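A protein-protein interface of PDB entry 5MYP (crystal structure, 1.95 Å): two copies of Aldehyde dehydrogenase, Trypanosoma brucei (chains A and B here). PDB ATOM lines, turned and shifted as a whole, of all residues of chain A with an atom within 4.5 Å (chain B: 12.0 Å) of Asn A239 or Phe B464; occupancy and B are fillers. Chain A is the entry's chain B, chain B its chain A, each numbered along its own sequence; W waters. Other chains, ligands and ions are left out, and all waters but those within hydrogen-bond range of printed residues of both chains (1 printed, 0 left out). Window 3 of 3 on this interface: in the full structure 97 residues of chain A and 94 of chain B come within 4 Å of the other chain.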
ATOM      1  N   THR A 235      -1.465   1.006 -19.561  1.00  0.00           N
ATOM      2  CA  THR A 235      -1.780  -0.427 -19.451  1.00  0.00           C
ATOM      3  C   THR A 235      -0.694  -1.220 -18.706  1.00  0.00           C
ATOM      4  O   THR A 235      -0.745  -2.450 -18.686  1.00  0.00           O
ATOM      5  CB  THR A 235      -2.021  -1.061 -20.843  1.00  0.00           C
ATOM      6  OG1 THR A 235      -0.823  -0.985 -21.630  1.00  0.00           O
ATOM      7  CG2 THR A 235      -3.156  -0.350 -21.571  1.00  0.00           C
ATOM      8  N   CYS A 236       0.258  -0.517 -18.077  1.00  0.00           N
ATOM      9  CA  CYS A 236       1.415  -1.135 -17.408  1.00  0.00           C
ATOM     10  C   CYS A 236       1.456  -0.925 -15.884  1.00  0.00           C
ATOM     11  O   CYS A 236       2.501  -1.158 -15.270  1.00  0.00           O
ATOM     12  CB  CYS A 236       2.724  -0.590 -18.006  1.00  0.00           C
ATOM     13  SG  CYS A 236       2.946  -0.894 -19.766  1.00  0.00           S
ATOM     14  N   ALA A 237       0.344  -0.521 -15.264  1.00  0.00           N
ATOM     15  CA  ALA A 237       0.313  -0.292 -13.806  1.00  0.00           C
ATOM     16  C   ALA A 237       0.848  -1.486 -13.007  1.00  0.00           C
ATOM     17  O   ALA A 237       1.665  -1.313 -12.105  1.00  0.00           O
ATOM     18  CB  ALA A 237      -1.097   0.060 -13.347  1.00  0.00           C
ATOM     19  N   ASP A 238       0.412  -2.689 -13.375  1.00  0.00           N
ATOM     20  CA  ASP A 238       0.837  -3.929 -12.709  1.00  0.00           C
ATOM     21  C   ASP A 238       2.289  -4.336 -13.012  1.00  0.00           C
ATOM     22  O   ASP A 238       2.859  -5.147 -12.280  1.00  0.00           O
ATOM     23  CB  ASP A 238      -0.091  -5.096 -13.089  1.00  0.00           C
ATOM     24  CG  ASP A 238      -1.542  -4.871 -12.670  1.00  0.00           C
ATOM     25  OD1 ASP A 238      -1.794  -4.134 -11.689  1.00  0.00           O
ATOM     26  OD2 ASP A 238      -2.438  -5.444 -13.333  1.00  0.00           O
ATOM     27  N   ASN A 239       2.866  -3.795 -14.088  1.00  0.00           N
ATOM     28  CA  ASN A 239       4.245  -4.081 -14.499  1.00  0.00           C
ATOM     29  C   ASN A 239       5.224  -2.936 -14.206  1.00  0.00           C
ATOM     30  O   ASN A 239       6.356  -2.957 -14.695  1.00  0.00           O
ATOM     31  CB  ASN A 239       4.277  -4.375 -16.005  1.00  0.00           C
ATOM     32  CG  ASN A 239       3.245  -5.403 -16.421  1.00  0.00           C
ATOM     33  OD1 ASN A 239       3.344  -6.575 -16.057  1.00  0.00           O
ATOM     34  ND2 ASN A 239       2.250  -4.969 -17.181  1.00  0.00           N
ATOM     35  N   MET A 240       4.805  -1.960 -13.397  1.00  0.00           N
ATOM     36  CA  MET A 240       5.533  -0.689 -13.277  1.00  0.00           C
ATOM     37  C   MET A 240       6.934  -0.840 -12.678  1.00  0.00           C
ATOM     38  O   MET A 240       7.832  -0.066 -13.015  1.00  0.00           O
ATOM     39  CB  MET A 240       4.706   0.334 -12.481  1.00  0.00           C
ATOM     40  CG  MET A 240       5.171   1.782 -12.607  1.00  0.00           C
ATOM     41  SD  MET A 240       5.229   2.436 -14.293  1.00  0.00           S
ATOM     42  CE  MET A 240       3.525   2.348 -14.805  1.00  0.00           C
ATOM     43  N   LYS A 241       7.127  -1.835 -11.812  1.00  0.00           N
ATOM     44  CA  LYS A 241       8.454  -2.115 -11.252  1.00  0.00           C
ATOM     45  C   LYS A 241       9.435  -2.584 -12.333  1.00  0.00           C
ATOM     46  O   LYS A 241      10.575  -2.122 -12.380  1.00  0.00           O
ATOM     47  CB  LYS A 241       8.379  -3.150 -10.127  1.00  0.00           C
ATOM     48  CG  LYS A 241       9.635  -3.198  -9.268  1.00  0.00           C
ATOM     49  CD  LYS A 241       9.439  -3.989  -7.979  1.00  0.00           C
ATOM     50  CE  LYS A 241       9.841  -5.446  -8.134  1.00  0.00           C
ATOM     51  NZ  LYS A 241      11.314  -5.627  -7.984  1.00  0.00           N
ATOM     52  N   VAL A 242       8.980  -3.491 -13.197  1.00  0.00           N
ATOM     53  CA  VAL A 242       9.807  -4.002 -14.300  1.00  0.00           C
ATOM     54  C   VAL A 242      10.032  -2.919 -15.365  1.00  0.00           C
ATOM     55  O   VAL A 242      11.127  -2.818 -15.916  1.00  0.00           O
ATOM     56  CB  VAL A 242       9.204  -5.285 -14.921  1.00  0.00           C
ATOM     57  CG1 VAL A 242       9.974  -5.715 -16.168  1.00  0.00           C
ATOM     58  CG2 VAL A 242       9.218  -6.414 -13.892  1.00  0.00           C
ATOM     59  N   VAL A 243       8.997  -2.126 -15.642  1.00  0.00           N
ATOM     60  CA  VAL A 243       9.102  -0.969 -16.548  1.00  0.00           C
ATOM     61  C   VAL A 243      10.228  -0.045 -16.079  1.00  0.00           C
ATOM     62  O   VAL A 243      11.117   0.298 -16.857  1.00  0.00           O
ATOM     63  CB  VAL A 243       7.770  -0.175 -16.640  1.00  0.00           C
ATOM     64  CG1 VAL A 243       7.957   1.165 -17.359  1.00  0.00           C
ATOM     65  CG2 VAL A 243       6.689  -0.994 -17.339  1.00  0.00           C
ATOM     66  N   ARG A 246      13.901  -1.625 -16.152  1.00  0.00           N
ATOM     67  CA  ARG A 246      14.465  -1.679 -17.504  1.00  0.00           C
ATOM     68  C   ARG A 246      14.909  -0.293 -17.987  1.00  0.00           C
ATOM     69  O   ARG A 246      16.014  -0.149 -18.509  1.00  0.00           O
ATOM     70  CB  ARG A 246      13.483  -2.337 -18.477  1.00  0.00           C
ATOM     71  CG  ARG A 246      13.350  -3.828 -18.202  1.00  0.00           C
ATOM     72  CD  ARG A 246      12.244  -4.508 -18.986  1.00  0.00           C
ATOM     73  NE  ARG A 246      12.170  -5.925 -18.625  1.00  0.00           N
ATOM     74  CZ  ARG A 246      11.394  -6.840 -19.209  1.00  0.00           C
ATOM     75  NH1 ARG A 246      10.592  -6.523 -20.228  1.00  0.00           N
ATOM     76  NH2 ARG A 246      11.427  -8.099 -18.761  1.00  0.00           N
ATOM     77  N   PHE A 398       6.506   1.055 -23.852  1.00  0.00           N
ATOM     78  CA  PHE A 398       6.031   0.153 -22.807  1.00  0.00           C
ATOM     79  C   PHE A 398       4.510   0.149 -22.830  1.00  0.00           C
ATOM     80  O   PHE A 398       3.882   1.181 -22.587  1.00  0.00           O
ATOM     81  CB  PHE A 398       6.572   0.568 -21.439  1.00  0.00           C
ATOM     82  CG  PHE A 398       8.031   0.263 -21.253  1.00  0.00           C
ATOM     83  CD1 PHE A 398       9.004   1.140 -21.723  1.00  0.00           C
ATOM     84  CD2 PHE A 398       8.436  -0.904 -20.615  1.00  0.00           C
ATOM     85  CE1 PHE A 398      10.352   0.862 -21.555  1.00  0.00           C
ATOM     86  CE2 PHE A 398       9.785  -1.190 -20.445  1.00  0.00           C
ATOM     87  CZ  PHE A 398      10.745  -0.305 -20.918  1.00  0.00           C
ATOM     88  N   ASN A 400       0.876  -2.940 -22.886  1.00  0.00           N
ATOM     89  CA  ASN A 400       0.241  -4.250 -23.075  1.00  0.00           C
ATOM     90  C   ASN A 400      -0.895  -4.189 -24.116  1.00  0.00           C
ATOM     91  O   ASN A 400      -1.623  -5.173 -24.294  1.00  0.00           O
ATOM     92  CB  ASN A 400      -0.302  -4.776 -21.733  1.00  0.00           C
ATOM     93  CG  ASN A 400       0.799  -5.149 -20.756  1.00  0.00           C
ATOM     94  OD1 ASN A 400       0.872  -4.614 -19.646  1.00  0.00           O
ATOM     95  ND2 ASN A 400       1.661  -6.067 -21.162  1.00  0.00           N
ATOM     96  N   ASN A 420       8.521  -2.903 -24.617  1.00  0.00           N
ATOM     97  CA  ASN A 420       8.683  -3.354 -23.224  1.00  0.00           C
ATOM     98  C   ASN A 420      10.124  -3.601 -22.770  1.00  0.00           C
ATOM     99  O   ASN A 420      10.354  -4.334 -21.809  1.00  0.00           O
ATOM    100  CB  ASN A 420       7.783  -4.570 -22.914  1.00  0.00           C
ATOM    101  CG  ASN A 420       6.307  -4.259 -23.088  1.00  0.00           C
ATOM    102  OD1 ASN A 420       5.858  -3.149 -22.810  1.00  0.00           O
ATOM    103  ND2 ASN A 420       5.544  -5.245 -23.541  1.00  0.00           N
ATOM    104  N   LEU B 108      13.955 -16.037 -28.529  1.00  0.00           N
ATOM    105  CA  LEU B 108      12.753 -16.136 -27.690  1.00  0.00           C
ATOM    106  C   LEU B 108      11.776 -14.955 -27.826  1.00  0.00           C
ATOM    107  O   LEU B 108      10.625 -15.071 -27.417  1.00  0.00           O
ATOM    108  CB  LEU B 108      13.152 -16.306 -26.221  1.00  0.00           C
ATOM    109  CG  LEU B 108      13.999 -17.542 -25.897  1.00  0.00           C
ATOM    110  CD1 LEU B 108      14.453 -17.512 -24.446  1.00  0.00           C
ATOM    111  CD2 LEU B 108      13.232 -18.821 -26.195  1.00  0.00           C
ATOM    112  N   ASP B 109      12.232 -13.833 -28.382  1.00  0.00           N
ATOM    113  CA  ASP B 109      11.379 -12.652 -28.576  1.00  0.00           C
ATOM    114  C   ASP B 109      10.723 -12.635 -29.953  1.00  0.00           C
ATOM    115  O   ASP B 109      11.099 -13.404 -30.844  1.00  0.00           O
ATOM    116  CB  ASP B 109      12.192 -11.370 -28.367  1.00  0.00           C
ATOM    117  CG  ASP B 109      12.801 -11.283 -26.984  1.00  0.00           C
ATOM    118  OD1 ASP B 109      12.096 -11.584 -25.996  1.00  0.00           O
ATOM    119  OD2 ASP B 109      13.986 -10.906 -26.881  1.00  0.00           O
ATOM    120  N   ASP B 110       9.728 -11.765 -30.099  1.00  0.00           N
ATOM    121  CA  ASP B 110       9.011 -11.576 -31.357  1.00  0.00           C
ATOM    122  C   ASP B 110       9.663 -10.433 -32.138  1.00  0.00           C
ATOM    123  O   ASP B 110       9.492  -9.258 -31.780  1.00  0.00           O
ATOM    124  CB  ASP B 110       7.533 -11.271 -31.073  1.00  0.00           C
ATOM    125  CG  ASP B 110       6.767 -10.815 -32.314  1.00  0.00           C
ATOM    126  OD1 ASP B 110       6.987 -11.403 -33.397  1.00  0.00           O
ATOM    127  OD2 ASP B 110       5.948  -9.875 -32.209  1.00  0.00           O
ATOM    128  N   MET B 460      11.618  -5.283 -32.143  1.00  0.00           N
ATOM    129  CA  MET B 460      11.726  -6.386 -31.184  1.00  0.00           C
ATOM    130  C   MET B 460      10.645  -6.215 -30.122  1.00  0.00           C
ATOM    131  O   MET B 460      10.617  -5.193 -29.438  1.00  0.00           O
ATOM    132  CB  MET B 460      13.108  -6.381 -30.522  1.00  0.00           C
ATOM    133  CG  MET B 460      13.227  -7.281 -29.295  1.00  0.00           C
ATOM    134  SD  MET B 460      14.870  -7.315 -28.577  1.00  0.00           S
ATOM    135  CE  MET B 460      15.655  -8.586 -29.559  1.00  0.00           C
ATOM    136  N   ARG B 461       9.777  -7.217 -29.971  1.00  0.00           N
ATOM    137  CA  ARG B 461       8.702  -7.166 -28.977  1.00  0.00           C
ATOM    138  C   ARG B 461       8.957  -8.186 -27.871  1.00  0.00           C
ATOM    139  O   ARG B 461       9.130  -9.384 -28.139  1.00  0.00           O
ATOM    140  CB  ARG B 461       7.342  -7.395 -29.638  1.00  0.00           C
ATOM    141  CG  ARG B 461       7.114  -6.510 -30.862  1.00  0.00           C
ATOM    142  CD  ARG B 461       5.641  -6.248 -31.138  1.00  0.00           C
ATOM    143  NE  ARG B 461       5.455  -5.521 -32.396  1.00  0.00           N
ATOM    144  CZ  ARG B 461       5.508  -6.062 -33.617  1.00  0.00           C
ATOM    145  NH1 ARG B 461       5.732  -7.373 -33.789  1.00  0.00           N
ATOM    146  NH2 ARG B 461       5.325  -5.277 -34.686  1.00  0.00           N
ATOM    147  N   ARG B 462       9.017  -7.692 -26.635  1.00  0.00           N
ATOM    148  CA  ARG B 462       9.267  -8.513 -25.457  1.00  0.00           C
ATOM    149  C   ARG B 462       8.074  -8.450 -24.513  1.00  0.00           C
ATOM    150  O   ARG B 462       7.196  -7.580 -24.646  1.00  0.00           O
ATOM    151  CB  ARG B 462      10.522  -8.026 -24.730  1.00  0.00           C
ATOM    152  CG  ARG B 462      11.751  -7.908 -25.626  1.00  0.00           C
ATOM    153  CD  ARG B 462      13.070  -7.837 -24.858  1.00  0.00           C
ATOM    154  NE  ARG B 462      13.048  -8.557 -23.578  1.00  0.00           N
ATOM    155  CZ  ARG B 462      13.614  -9.738 -23.313  1.00  0.00           C
ATOM    156  NH1 ARG B 462      14.323 -10.416 -24.220  1.00  0.00           N
ATOM    157  NH2 ARG B 462      13.480 -10.253 -22.095  1.00  0.00           N
ATOM    158  N   GLY B 463       8.048  -9.387 -23.565  1.00  0.00           N
ATOM    159  CA  GLY B 463       7.072  -9.397 -22.476  1.00  0.00           C
ATOM    160  C   GLY B 463       7.716  -8.921 -21.188  1.00  0.00           C
ATOM    161  O   GLY B 463       8.906  -8.606 -21.163  1.00  0.00           O
ATOM    162  N   PHE B 464       6.931  -8.902 -20.114  1.00  0.00           N
ATOM    163  CA  PHE B 464       7.411  -8.469 -18.797  1.00  0.00           C
ATOM    164  C   PHE B 464       7.941  -9.603 -17.904  1.00  0.00           C
ATOM    165  O   PHE B 464       8.318  -9.354 -16.759  1.00  0.00           O
ATOM    166  CB  PHE B 464       6.300  -7.695 -18.078  1.00  0.00           C
ATOM    167  CG  PHE B 464       6.021  -6.352 -18.680  1.00  0.00           C
ATOM    168  CD1 PHE B 464       6.939  -5.318 -18.535  1.00  0.00           C
ATOM    169  CD2 PHE B 464       4.847  -6.110 -19.383  1.00  0.00           C
ATOM    170  CE1 PHE B 464       6.698  -4.069 -19.084  1.00  0.00           C
ATOM    171  CE2 PHE B 464       4.598  -4.859 -19.931  1.00  0.00           C
ATOM    172  CZ  PHE B 464       5.526  -3.838 -19.779  1.00  0.00           C
ATOM    173  N   LEU B 465       8.006 -10.825 -18.433  1.00  0.00           N
ATOM    174  CA  LEU B 465       8.516 -11.973 -17.679  1.00  0.00           C
ATOM    175  C   LEU B 465      10.044 -11.968 -17.636  1.00  0.00           C
ATOM    176  O   LEU B 465      10.701 -11.266 -18.409  1.00  0.00           O
ATOM    177  CB  LEU B 465       8.020 -13.298 -18.282  1.00  0.00           C
ATOM    178  CG  LEU B 465       6.573 -13.715 -18.013  1.00  0.00           C
ATOM    179  CD1 LEU B 465       5.578 -12.713 -18.579  1.00  0.00           C
ATOM    180  CD2 LEU B 465       6.355 -15.104 -18.598  1.00  0.00           C
ATOM    181  N   PHE B 466      10.590 -12.769 -16.724  1.00  0.00           N
ATOM    182  CA  PHE B 466      12.032 -12.959 -16.576  1.00  0.00           C
ATOM    183  C   PHE B 466      12.611 -13.689 -17.791  1.00  0.00           C
ATOM    184  O   PHE B 466      11.931 -14.511 -18.404  1.00  0.00           O
ATOM    185  CB  PHE B 466      12.312 -13.770 -15.302  1.00  0.00           C
ATOM    186  CG  PHE B 466      13.755 -13.782 -14.883  1.00  0.00           C
ATOM    187  CD1 PHE B 466      14.245 -12.813 -14.012  1.00  0.00           C
ATOM    188  CD2 PHE B 466      14.622 -14.776 -15.333  1.00  0.00           C
ATOM    189  CE1 PHE B 466      15.573 -12.826 -13.609  1.00  0.00           C
ATOM    190  CE2 PHE B 466      15.953 -14.792 -14.934  1.00  0.00           C
ATOM    191  CZ  PHE B 466      16.429 -13.815 -14.070  1.00  0.00           C
ATOM    192  N   SER B 467      13.855 -13.365 -18.140  1.00  0.00           N
ATOM    193  CA  SER B 467      14.597 -14.082 -19.183  1.00  0.00           C
ATOM    194  C   SER B 467      16.103 -14.059 -18.887  1.00  0.00           C
ATOM    195  O   SER B 467      16.543 -13.383 -17.954  1.00  0.00           O
ATOM    196  CB  SER B 467      14.281 -13.507 -20.573  1.00  0.00           C
ATOM    197  OG  SER B 467      14.894 -12.253 -20.785  1.00  0.00           O
ATOM    198  N   SER B 468      16.876 -14.795 -19.685  1.00  0.00           N
ATOM    199  CA  SER B 468      18.309 -15.028 -19.426  1.00  0.00           C
ATOM    200  C   SER B 468      19.169 -13.766 -19.269  1.00  0.00           C
ATOM    201  O   SER B 468      20.130 -13.774 -18.501  1.00  0.00           O
ATOM    202  CB  SER B 468      18.908 -15.916 -20.520  1.00  0.00           C
ATOM    203  OG  SER B 468      18.706 -15.355 -21.804  1.00  0.00           O
ATOM    204  N   ILE B 469      18.834 -12.701 -19.996  1.00  0.00           N
ATOM    205  CA  ILE B 469      19.538 -11.409 -19.859  1.00  0.00           C
ATOM    206  C   ILE B 469      19.416 -10.804 -18.450  1.00  0.00           C
ATOM    207  O   ILE B 469      20.359 -10.170 -17.965  1.00  0.00           O
ATOM    208  CB  ILE B 469      19.091 -10.362 -20.919  1.00  0.00           C
ATOM    209  CG1 ILE B 469      17.619  -9.948 -20.728  1.00  0.00           C
ATOM    210  CG2 ILE B 469      19.355 -10.886 -22.331  1.00  0.00           C
ATOM    211  CD1 ILE B 469      17.062  -9.080 -21.835  1.00  0.00           C
ATOM    212  N   ASP B 470      18.273 -11.033 -17.796  1.00  0.00           N
ATOM    213  CA  ASP B 470      18.002 -10.492 -16.453  1.00  0.00           C
ATOM    214  C   ASP B 470      18.840 -11.115 -15.332  1.00  0.00           C
ATOM    215  O   ASP B 470      18.906 -10.552 -14.237  1.00  0.00           O
ATOM    216  CB  ASP B 470      16.517 -10.638 -16.092  1.00  0.00           C
ATOM    217  CG  ASP B 470      15.595  -9.915 -17.064  1.00  0.00           C
ATOM    218  OD1 ASP B 470      15.928  -8.794 -17.499  1.00  0.00           O
ATOM    219  OD2 ASP B 470      14.526 -10.466 -17.379  1.00  0.00           O
ATOM    220  N   THR B 471      19.465 -12.269 -15.591  1.00  0.00           N
ATOM    221  CA  THR B 471      20.361 -12.907 -14.615  1.00  0.00           C
ATOM    222  C   THR B 471      21.668 -12.133 -14.395  1.00  0.00           C
ATOM    223  O   THR B 471      22.289 -12.277 -13.340  1.00  0.00           O
ATOM    224  CB  THR B 471      20.733 -14.354 -15.016  1.00  0.00           C
ATOM    225  OG1 THR B 471      21.388 -14.350 -16.291  1.00  0.00           O
ATOM    226  CG2 THR B 471      19.496 -15.255 -15.066  1.00  0.00           C
ATOM    227  N   ARG B 473      22.357  -8.561 -16.279  1.00  0.00           N
ATOM    228  CA  ARG B 473      22.428  -7.156 -16.716  1.00  0.00           C
ATOM    229  C   ARG B 473      22.303  -6.114 -15.589  1.00  0.00           C
ATOM    230  O   ARG B 473      22.976  -5.083 -15.640  1.00  0.00           O
ATOM    231  CB  ARG B 473      21.429  -6.856 -17.852  1.00  0.00           C
ATOM    232  CG  ARG B 473      19.947  -6.871 -17.490  1.00  0.00           C
ATOM    233  CD  ARG B 473      19.118  -6.194 -18.581  1.00  0.00           C
ATOM    234  NE  ARG B 473      17.743  -6.698 -18.649  1.00  0.00           N
ATOM    235  CZ  ARG B 473      16.755  -6.156 -19.364  1.00  0.00           C
ATOM    236  NH1 ARG B 473      15.547  -6.713 -19.348  1.00  0.00           N
ATOM    237  NH2 ARG B 473      16.950  -5.053 -20.085  1.00  0.00           N
ATOM    238  N   PHE B 474      21.475  -6.388 -14.578  1.00  0.00           N
ATOM    239  CA  PHE B 474      21.132  -5.374 -13.568  1.00  0.00           C
ATOM    240  C   PHE B 474      22.179  -5.232 -12.468  1.00  0.00           C
ATOM    241  O   PHE B 474      22.562  -6.232 -11.855  1.00  0.00           O
ATOM    242  CB  PHE B 474      19.780  -5.689 -12.918  1.00  0.00           C
ATOM    243  CG  PHE B 474      18.622  -5.651 -13.876  1.00  0.00           C
ATOM    244  CD1 PHE B 474      18.298  -4.476 -14.543  1.00  0.00           C
ATOM    245  CD2 PHE B 474      17.844  -6.784 -14.102  1.00  0.00           C
ATOM    246  CE1 PHE B 474      17.230  -4.431 -15.431  1.00  0.00           C
ATOM    247  CE2 PHE B 474      16.773  -6.743 -14.984  1.00  0.00           C
ATOM    248  CZ  PHE B 474      16.466  -5.566 -15.653  1.00  0.00           C
HETATM  249  O   HOH W   1      13.706  -7.316 -16.265  1.00  0.00           O
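The guanidinium group of Arg B462 sits at hydrogen-bond distance from the side-chain hydroxyl of Ser B467, 2.8 Å away.
The backbone carbonyl oxygen of Thr A235 sits close to the side-chain amide oxygen of Asn A400, 2.9 Å away.
The side-chain sulfur of Cys A236 sits close to the backbone carbonyl oxygen of Phe A398, 3.6 Å away.
The guanidinium group of Arg A246 is in hydrogen-bond range of the backbone carbonyl oxygen of Asn A420, 2.7 Å away.
The side-chain amide oxygen of Asn A400 lies within hydrogen-bond range of the side-chain amide nitrogen of Asn A239.
The guanidinium group (NH1) of Arg B462 lies within salt-bridge range of the side-chain carboxylate (OD2) of Asp B109 (2.7 Å).
The backbone carbonyl oxygen (O) of Gly B463 lies within hydrogen-bond range of the guanidinium group (NH1) of Arg A246, at 2.8 Å.
O of Arg B462 lies within hydrogen-bond range of ND2 of Asn A420, 3.1 Å away.
The guanidinium group (NH2) of Arg A246 is in hydrogen-bond range of the backbone carbonyl oxygen (O) of Leu B465.
SG of Cys A236 touches CZ of Phe B464, at 3.9 Å.
CD2 of Phe B464 touches CG of Asn A239 (3.4 Å).
CD1 of Phe B464 touches CG1 of Val A242, at 3.9 Å.
Val A243 touches Phe B464 (CG2 to CE1, 3.5 Å).
Arg A246 touches Phe B464 (NH2 to C, 3.9 Å).
Arg A246 touches Arg B473 (NE to NH1, 3.5 Å).
Phe A398 touches Phe B464 (CD2 to CE1, 3.9 Å).
Asn A400 touches Phe B464.
Asn A420 touches Phe B464.
No position is printed for both chains.
Water W1 bridges OD1 of Asp B470 (2.9 Å) and NE of Arg A246 (3.1 Å).
Asn A239 touches just one residue of chain B: Phe B464.
Printed residues of chain A within 4 Å of Phe B464: Cys A236 (3.9 Å), Asn A239 (3.4 Å), Val A242 (3.9 Å), Val A243 (3.5 Å), Arg A246 (3.9 Å), Phe A398 (3.9 Å), Asn A400 (3.4 Å) and Asn A420 (3.1 Å).
No residue of chain B comes within 4 Å of Ala A237.
No residue of chain B comes within 4 Å of Asp A238.
Met A240 touches none of the printed residues of chain B.
Of chain B, only Phe B464 (3.5 Å) comes within 4 Å of Val A243.
Phe A398 touches just one residue of chain B: Phe B464.
Of chain B, only Phe B464 comes within 4 Å of Asn A400.
Asn A420 touches just these residues of chain B: Arg B462 (3.1 Å) and Phe B464 (3.1 Å).
Printed residues of chain B within 4 Å of Arg A246: Gly B463, Phe B464, Leu B465 and Arg B473.
Of the printed residues of chain A, Arg B473 touches Arg A246 (3.5 Å).
Of the printed residues of chain A, Gly B463 touches Arg A246 (2.8 Å).
Leu B108 touches none of the printed residues of chain A.
The nearest printed residue of chain A that does not touch Phe B464 is Thr A235 (6.0 Å).
The nearest printed residue of chain A that does not touch Arg B473 is Asn A420 (6.2 Å).
Hydrophobic or aromatic side chains of chain A that line the printed part of chain B: Val A242, Val A243 and Phe A398.
Printed residues of chain B that touch a printed residue of chain A: Arg B462, Gly B463, Phe B464, Leu B465 and Arg B473.
Among the printed residues, no Asp or Glu carboxylate lies within 4 Å of a Lys or Arg side-chain nitrogen of the other chain.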
